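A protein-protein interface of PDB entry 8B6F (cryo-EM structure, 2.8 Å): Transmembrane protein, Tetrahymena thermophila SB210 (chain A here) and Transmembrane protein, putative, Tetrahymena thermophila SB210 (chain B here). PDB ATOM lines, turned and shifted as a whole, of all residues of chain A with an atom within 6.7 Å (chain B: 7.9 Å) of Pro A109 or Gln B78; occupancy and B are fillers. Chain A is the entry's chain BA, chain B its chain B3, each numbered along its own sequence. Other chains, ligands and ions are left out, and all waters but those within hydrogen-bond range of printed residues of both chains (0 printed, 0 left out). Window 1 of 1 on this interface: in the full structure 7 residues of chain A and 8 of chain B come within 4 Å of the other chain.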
ATOM      1  N   MET A 103      23.688 -27.831 -11.382  1.00  0.00           N
ATOM      2  CA  MET A 103      23.872 -26.393 -11.546  1.00  0.00           C
ATOM      3  C   MET A 103      25.348 -26.023 -11.513  1.00  0.00           C
ATOM      4  O   MET A 103      25.800 -25.170 -12.286  1.00  0.00           O
ATOM      5  CB  MET A 103      23.108 -25.638 -10.458  1.00  0.00           C
ATOM      6  CG  MET A 103      21.599 -25.634 -10.655  1.00  0.00           C
ATOM      7  SD  MET A 103      20.742 -24.525  -9.519  1.00  0.00           S
ATOM      8  CE  MET A 103      21.109 -25.295  -7.947  1.00  0.00           C
ATOM      9  N   GLU A 106      26.850 -27.073 -14.930  1.00  0.00           N
ATOM     10  CA  GLU A 106      26.407 -26.292 -16.073  1.00  0.00           C
ATOM     11  C   GLU A 106      27.110 -24.938 -16.103  1.00  0.00           C
ATOM     12  O   GLU A 106      27.613 -24.464 -15.082  1.00  0.00           O
ATOM     13  CB  GLU A 106      24.899 -26.059 -16.030  1.00  0.00           C
ATOM     14  CG  GLU A 106      24.062 -27.279 -16.325  1.00  0.00           C
ATOM     15  CD  GLU A 106      22.677 -26.938 -16.837  1.00  0.00           C
ATOM     16  OE1 GLU A 106      22.326 -25.740 -16.870  1.00  0.00           O
ATOM     17  OE2 GLU A 106      21.935 -27.872 -17.208  1.00  0.00           O
ATOM     18  N   PRO A 107      27.163 -24.296 -17.269  1.00  0.00           N
ATOM     19  CA  PRO A 107      27.618 -22.903 -17.309  1.00  0.00           C
ATOM     20  C   PRO A 107      26.703 -22.020 -16.476  1.00  0.00           C
ATOM     21  O   PRO A 107      25.489 -22.225 -16.425  1.00  0.00           O
ATOM     22  CB  PRO A 107      27.547 -22.542 -18.798  1.00  0.00           C
ATOM     23  CG  PRO A 107      27.548 -23.842 -19.515  1.00  0.00           C
ATOM     24  CD  PRO A 107      26.863 -24.817 -18.613  1.00  0.00           C
ATOM     25  N   LEU A 108      27.294 -21.035 -15.820  1.00  0.00           N
ATOM     26  CA  LEU A 108      26.507 -20.129 -14.998  1.00  0.00           C
ATOM     27  C   LEU A 108      25.587 -19.301 -15.890  1.00  0.00           C
ATOM     28  O   LEU A 108      26.062 -18.676 -16.846  1.00  0.00           O
ATOM     29  CB  LEU A 108      27.424 -19.218 -14.187  1.00  0.00           C
ATOM     30  CG  LEU A 108      26.839 -18.625 -12.903  1.00  0.00           C
ATOM     31  CD1 LEU A 108      26.579 -19.717 -11.879  1.00  0.00           C
ATOM     32  CD2 LEU A 108      27.758 -17.564 -12.329  1.00  0.00           C
ATOM     33  N   PRO A 109      24.279 -19.270 -15.627  1.00  0.00           N
ATOM     34  CA  PRO A 109      23.373 -18.537 -16.519  1.00  0.00           C
ATOM     35  C   PRO A 109      23.720 -17.057 -16.579  1.00  0.00           C
ATOM     36  O   PRO A 109      24.150 -16.454 -15.594  1.00  0.00           O
ATOM     37  CB  PRO A 109      21.991 -18.767 -15.897  1.00  0.00           C
ATOM     38  CG  PRO A 109      22.256 -19.132 -14.489  1.00  0.00           C
ATOM     39  CD  PRO A 109      23.558 -19.868 -14.490  1.00  0.00           C
ATOM     40  N   LEU A 110      23.528 -16.477 -17.759  1.00  0.00           N
ATOM     41  CA  LEU A 110      23.817 -15.067 -17.961  1.00  0.00           C
ATOM     42  C   LEU A 110      22.794 -14.204 -17.227  1.00  0.00           C
ATOM     43  O   LEU A 110      21.687 -14.642 -16.904  1.00  0.00           O
ATOM     44  CB  LEU A 110      23.826 -14.736 -19.453  1.00  0.00           C
ATOM     45  CG  LEU A 110      24.847 -15.527 -20.276  1.00  0.00           C
ATOM     46  CD1 LEU A 110      24.640 -15.289 -21.759  1.00  0.00           C
ATOM     47  CD2 LEU A 110      26.269 -15.169 -19.871  1.00  0.00           C
ATOM     48  N   GLY A 111      23.181 -12.954 -16.969  1.00  0.00           N
ATOM     49  CA  GLY A 111      22.412 -12.056 -16.140  1.00  0.00           C
ATOM     50  C   GLY A 111      22.031 -10.771 -16.856  1.00  0.00           C
ATOM     51  O   GLY A 111      22.323 -10.567 -18.036  1.00  0.00           O
ATOM     52  N   TYR A 115      22.920  -9.155 -20.640  1.00  0.00           N
ATOM     53  CA  TYR A 115      21.863  -8.890 -21.610  1.00  0.00           C
ATOM     54  C   TYR A 115      21.767  -7.405 -21.930  1.00  0.00           C
ATOM     55  O   TYR A 115      21.628  -7.021 -23.096  1.00  0.00           O
ATOM     56  CB  TYR A 115      20.524  -9.420 -21.097  1.00  0.00           C
ATOM     57  CG  TYR A 115      20.346 -10.900 -21.334  1.00  0.00           C
ATOM     58  CD1 TYR A 115      19.857 -11.374 -22.545  1.00  0.00           C
ATOM     59  CD2 TYR A 115      20.679 -11.824 -20.355  1.00  0.00           C
ATOM     60  CE1 TYR A 115      19.698 -12.727 -22.770  1.00  0.00           C
ATOM     61  CE2 TYR A 115      20.525 -13.179 -20.570  1.00  0.00           C
ATOM     62  CZ  TYR A 115      20.032 -13.624 -21.780  1.00  0.00           C
ATOM     63  OH  TYR A 115      19.879 -14.973 -21.998  1.00  0.00           O
ATOM     64  N   ASN A 164      32.713 -15.423 -15.116  1.00  0.00           N
ATOM     65  CA  ASN A 164      31.919 -16.353 -14.320  1.00  0.00           C
ATOM     66  C   ASN A 164      32.633 -17.690 -14.179  1.00  0.00           C
ATOM     67  O   ASN A 164      32.809 -18.201 -13.068  1.00  0.00           O
ATOM     68  CB  ASN A 164      30.545 -16.551 -14.961  1.00  0.00           C
ATOM     69  CG  ASN A 164      29.733 -15.276 -15.011  1.00  0.00           C
ATOM     70  OD1 ASN A 164      30.257 -14.185 -14.793  1.00  0.00           O
ATOM     71  ND2 ASN A 164      28.447 -15.407 -15.307  1.00  0.00           N
ATOM     72  N   GLN A 169      32.405 -20.565 -10.898  1.00  0.00           N
ATOM     73  CA  GLN A 169      32.225 -21.987 -11.163  1.00  0.00           C
ATOM     74  C   GLN A 169      33.492 -22.784 -10.875  1.00  0.00           C
ATOM     75  O   GLN A 169      33.419 -23.905 -10.361  1.00  0.00           O
ATOM     76  CB  GLN A 169      31.778 -22.197 -12.610  1.00  0.00           C
ATOM     77  CG  GLN A 169      30.399 -21.635 -12.920  1.00  0.00           C
ATOM     78  CD  GLN A 169      29.301 -22.289 -12.099  1.00  0.00           C
ATOM     79  OE1 GLN A 169      29.145 -22.009 -10.912  1.00  0.00           O
ATOM     80  NE2 GLN A 169      28.535 -23.168 -12.732  1.00  0.00           N
ATOM     81  N   TYR B  70      17.428 -10.149  -8.400  1.00  0.00           N
ATOM     82  CA  TYR B  70      16.864 -11.405  -8.881  1.00  0.00           C
ATOM     83  C   TYR B  70      17.935 -12.300  -9.482  1.00  0.00           C
ATOM     84  O   TYR B  70      17.968 -13.507  -9.216  1.00  0.00           O
ATOM     85  CB  TYR B  70      15.772 -11.140  -9.915  1.00  0.00           C
ATOM     86  CG  TYR B  70      15.483 -12.349 -10.772  1.00  0.00           C
ATOM     87  CD1 TYR B  70      14.666 -13.373 -10.311  1.00  0.00           C
ATOM     88  CD2 TYR B  70      16.042 -12.474 -12.037  1.00  0.00           C
ATOM     89  CE1 TYR B  70      14.408 -14.484 -11.092  1.00  0.00           C
ATOM     90  CE2 TYR B  70      15.791 -13.578 -12.823  1.00  0.00           C
ATOM     91  CZ  TYR B  70      14.973 -14.580 -12.347  1.00  0.00           C
ATOM     92  OH  TYR B  70      14.720 -15.683 -13.127  1.00  0.00           O
ATOM     93  N   ASP B  71      18.827 -11.731 -10.292  1.00  0.00           N
ATOM     94  CA  ASP B  71      19.859 -12.540 -10.928  1.00  0.00           C
ATOM     95  C   ASP B  71      20.755 -13.208  -9.895  1.00  0.00           C
ATOM     96  O   ASP B  71      21.129 -14.376 -10.054  1.00  0.00           O
ATOM     97  CB  ASP B  71      20.691 -11.679 -11.877  1.00  0.00           C
ATOM     98  CG  ASP B  71      19.981 -11.401 -13.184  1.00  0.00           C
ATOM     99  OD1 ASP B  71      19.228 -12.278 -13.654  1.00  0.00           O
ATOM    100  OD2 ASP B  71      20.174 -10.305 -13.746  1.00  0.00           O
ATOM    101  N   TYR B  74      17.765 -15.638  -7.372  1.00  0.00           N
ATOM    102  CA  TYR B  74      17.102 -16.727  -8.075  1.00  0.00           C
ATOM    103  C   TYR B  74      17.627 -16.946  -9.486  1.00  0.00           C
ATOM    104  O   TYR B  74      17.234 -17.926 -10.127  1.00  0.00           O
ATOM    105  CB  TYR B  74      15.588 -16.475  -8.143  1.00  0.00           C
ATOM    106  CG  TYR B  74      14.864 -16.713  -6.836  1.00  0.00           C
ATOM    107  CD1 TYR B  74      14.418 -17.982  -6.489  1.00  0.00           C
ATOM    108  CD2 TYR B  74      14.617 -15.669  -5.956  1.00  0.00           C
ATOM    109  CE1 TYR B  74      13.753 -18.206  -5.299  1.00  0.00           C
ATOM    110  CE2 TYR B  74      13.953 -15.882  -4.762  1.00  0.00           C
ATOM    111  CZ  TYR B  74      13.523 -17.152  -4.441  1.00  0.00           C
ATOM    112  OH  TYR B  74      12.862 -17.371  -3.257  1.00  0.00           O
ATOM    113  N   GLY B  75      18.497 -16.068  -9.986  1.00  0.00           N
ATOM    114  CA  GLY B  75      19.024 -16.247 -11.326  1.00  0.00           C
ATOM    115  C   GLY B  75      19.811 -17.529 -11.488  1.00  0.00           C
ATOM    116  O   GLY B  75      19.815 -18.127 -12.567  1.00  0.00           O
ATOM    117  N   PHE B  76      20.490 -17.968 -10.428  1.00  0.00           N
ATOM    118  CA  PHE B  76      21.253 -19.208 -10.504  1.00  0.00           C
ATOM    119  C   PHE B  76      20.352 -20.392 -10.822  1.00  0.00           C
ATOM    120  O   PHE B  76      20.703 -21.250 -11.639  1.00  0.00           O
ATOM    121  CB  PHE B  76      21.993 -19.452  -9.189  1.00  0.00           C
ATOM    122  CG  PHE B  76      23.012 -18.402  -8.857  1.00  0.00           C
ATOM    123  CD1 PHE B  76      24.314 -18.518  -9.308  1.00  0.00           C
ATOM    124  CD2 PHE B  76      22.672 -17.307  -8.082  1.00  0.00           C
ATOM    125  CE1 PHE B  76      25.258 -17.559  -9.000  1.00  0.00           C
ATOM    126  CE2 PHE B  76      23.611 -16.343  -7.770  1.00  0.00           C
ATOM    127  CZ  PHE B  76      24.906 -16.471  -8.230  1.00  0.00           C
ATOM    128  N   THR B  77      19.186 -20.452 -10.185  1.00  0.00           N
ATOM    129  CA  THR B  77      18.297 -21.611 -10.296  1.00  0.00           C
ATOM    130  C   THR B  77      17.264 -21.404 -11.407  1.00  0.00           C
ATOM    131  O   THR B  77      16.057 -21.357 -11.178  1.00  0.00           O
ATOM    132  CB  THR B  77      17.621 -21.891  -8.956  1.00  0.00           C
ATOM    133  OG1 THR B  77      16.644 -22.928  -9.118  1.00  0.00           O
ATOM    134  CG2 THR B  77      16.937 -20.641  -8.401  1.00  0.00           C
ATOM    135  N   GLN B  78      17.768 -21.285 -12.633  1.00  0.00           N
ATOM    136  CA  GLN B  78      16.928 -21.252 -13.820  1.00  0.00           C
ATOM    137  C   GLN B  78      17.514 -22.186 -14.869  1.00  0.00           C
ATOM    138  O   GLN B  78      18.722 -22.435 -14.895  1.00  0.00           O
ATOM    139  CB  GLN B  78      16.793 -19.831 -14.390  1.00  0.00           C
ATOM    140  CG  GLN B  78      18.046 -19.281 -15.049  1.00  0.00           C
ATOM    141  CD  GLN B  78      17.858 -17.858 -15.539  1.00  0.00           C
ATOM    142  OE1 GLN B  78      16.878 -17.197 -15.200  1.00  0.00           O
ATOM    143  NE2 GLN B  78      18.797 -17.381 -16.348  1.00  0.00           N
ATOM    144  N   VAL B  79      16.644 -22.707 -15.731  1.00  0.00           N
ATOM    145  CA  VAL B  79      17.012 -23.700 -16.733  1.00  0.00           C
ATOM    146  C   VAL B  79      16.873 -23.072 -18.111  1.00  0.00           C
ATOM    147  O   VAL B  79      15.845 -22.459 -18.423  1.00  0.00           O
ATOM    148  CB  VAL B  79      16.148 -24.970 -16.614  1.00  0.00           C
ATOM    149  CG1 VAL B  79      16.307 -25.589 -15.238  1.00  0.00           C
ATOM    150  CG2 VAL B  79      14.682 -24.665 -16.893  1.00  0.00           C
ATOM    151  N   ASP B  80      17.914 -23.209 -18.927  1.00  0.00           N
ATOM    152  CA  ASP B  80      17.880 -22.671 -20.278  1.00  0.00           C
ATOM    153  C   ASP B  80      16.834 -23.400 -21.111  1.00  0.00           C
ATOM    154  O   ASP B  80      16.714 -24.627 -21.052  1.00  0.00           O
ATOM    155  CB  ASP B  80      19.257 -22.796 -20.931  1.00  0.00           C
ATOM    156  CG  ASP B  80      19.330 -22.104 -22.276  1.00  0.00           C
ATOM    157  OD1 ASP B  80      18.339 -21.451 -22.667  1.00  0.00           O
ATOM    158  OD2 ASP B  80      20.379 -22.211 -22.944  1.00  0.00           O
ATOM    159  N   ALA B  81      16.073 -22.637 -21.891  1.00  0.00           N
ATOM    160  CA  ALA B  81      15.031 -23.175 -22.764  1.00  0.00           C
ATOM    161  C   ALA B  81      15.326 -22.714 -24.187  1.00  0.00           C
ATOM    162  O   ALA B  81      15.006 -21.580 -24.557  1.00  0.00           O
ATOM    163  CB  ALA B  81      13.647 -22.725 -22.307  1.00  0.00           C
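The backbone carbonyl oxygen (O) of Tyr B70 sits at hydrogen-bond distance from the backbone NH (N) of Gly B75, at 2.7 Å. The side-chain amide oxygen (OE1) of Gln B78 sits at hydrogen-bond distance from the side-chain hydroxyl (OH) of Tyr B70, at 3.4 Å. O of Met A103 sits at hydrogen-bond distance from NE2 of Gln A169, 3.4 Å away.
Phe B76 touches Met A103 (O to SD, 3.9 Å). CA of Thr B77 touches SD of Met A103, at 3.9 Å. Phe B76 touches Leu A108. O of Gly B75 touches CG of Pro A109 (3.3 Å). O of Phe B76 touches CG of Pro A109, 3.9 Å away. Pro A109 touches Gln B78. Asp B71 touches Gly A111 (OD2 to C, 3.7 Å).
Pro A109 touches three residues of chain B. Of chain A, only Pro A109 (3.5 Å) comes within 4 Å of Gln B78. Of the printed residues of chain A, Asp B71 touches Gly A111 (3.7 Å). Printed residues of chain A within 4 Å of Thr B77: Met A103. The nearest residue of chain A that does not touch Gln B78 is Leu A110 (4.02 Å). The nearest printed residue of chain B that does not touch Met A103 is Gln B78 (5.4 Å).
Of the 10 printed residues of chain B, 5 touch a printed residue of chain A. Printed residues of chain A that touch a printed residue of chain B: Met A103, Leu A108, Pro A109 and Gly A111. Hydrophobic or aromatic side chains of chain A within 4 Å of the printed part of chain B: Met A103, Leu A108 and Pro A109. Among the printed residues, 7 pairs touch across the chains. Among the printed residues, no Asp or Glu carboxylate lies within 4 Å of a Lys or Arg side-chain nitrogen of the other chain.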
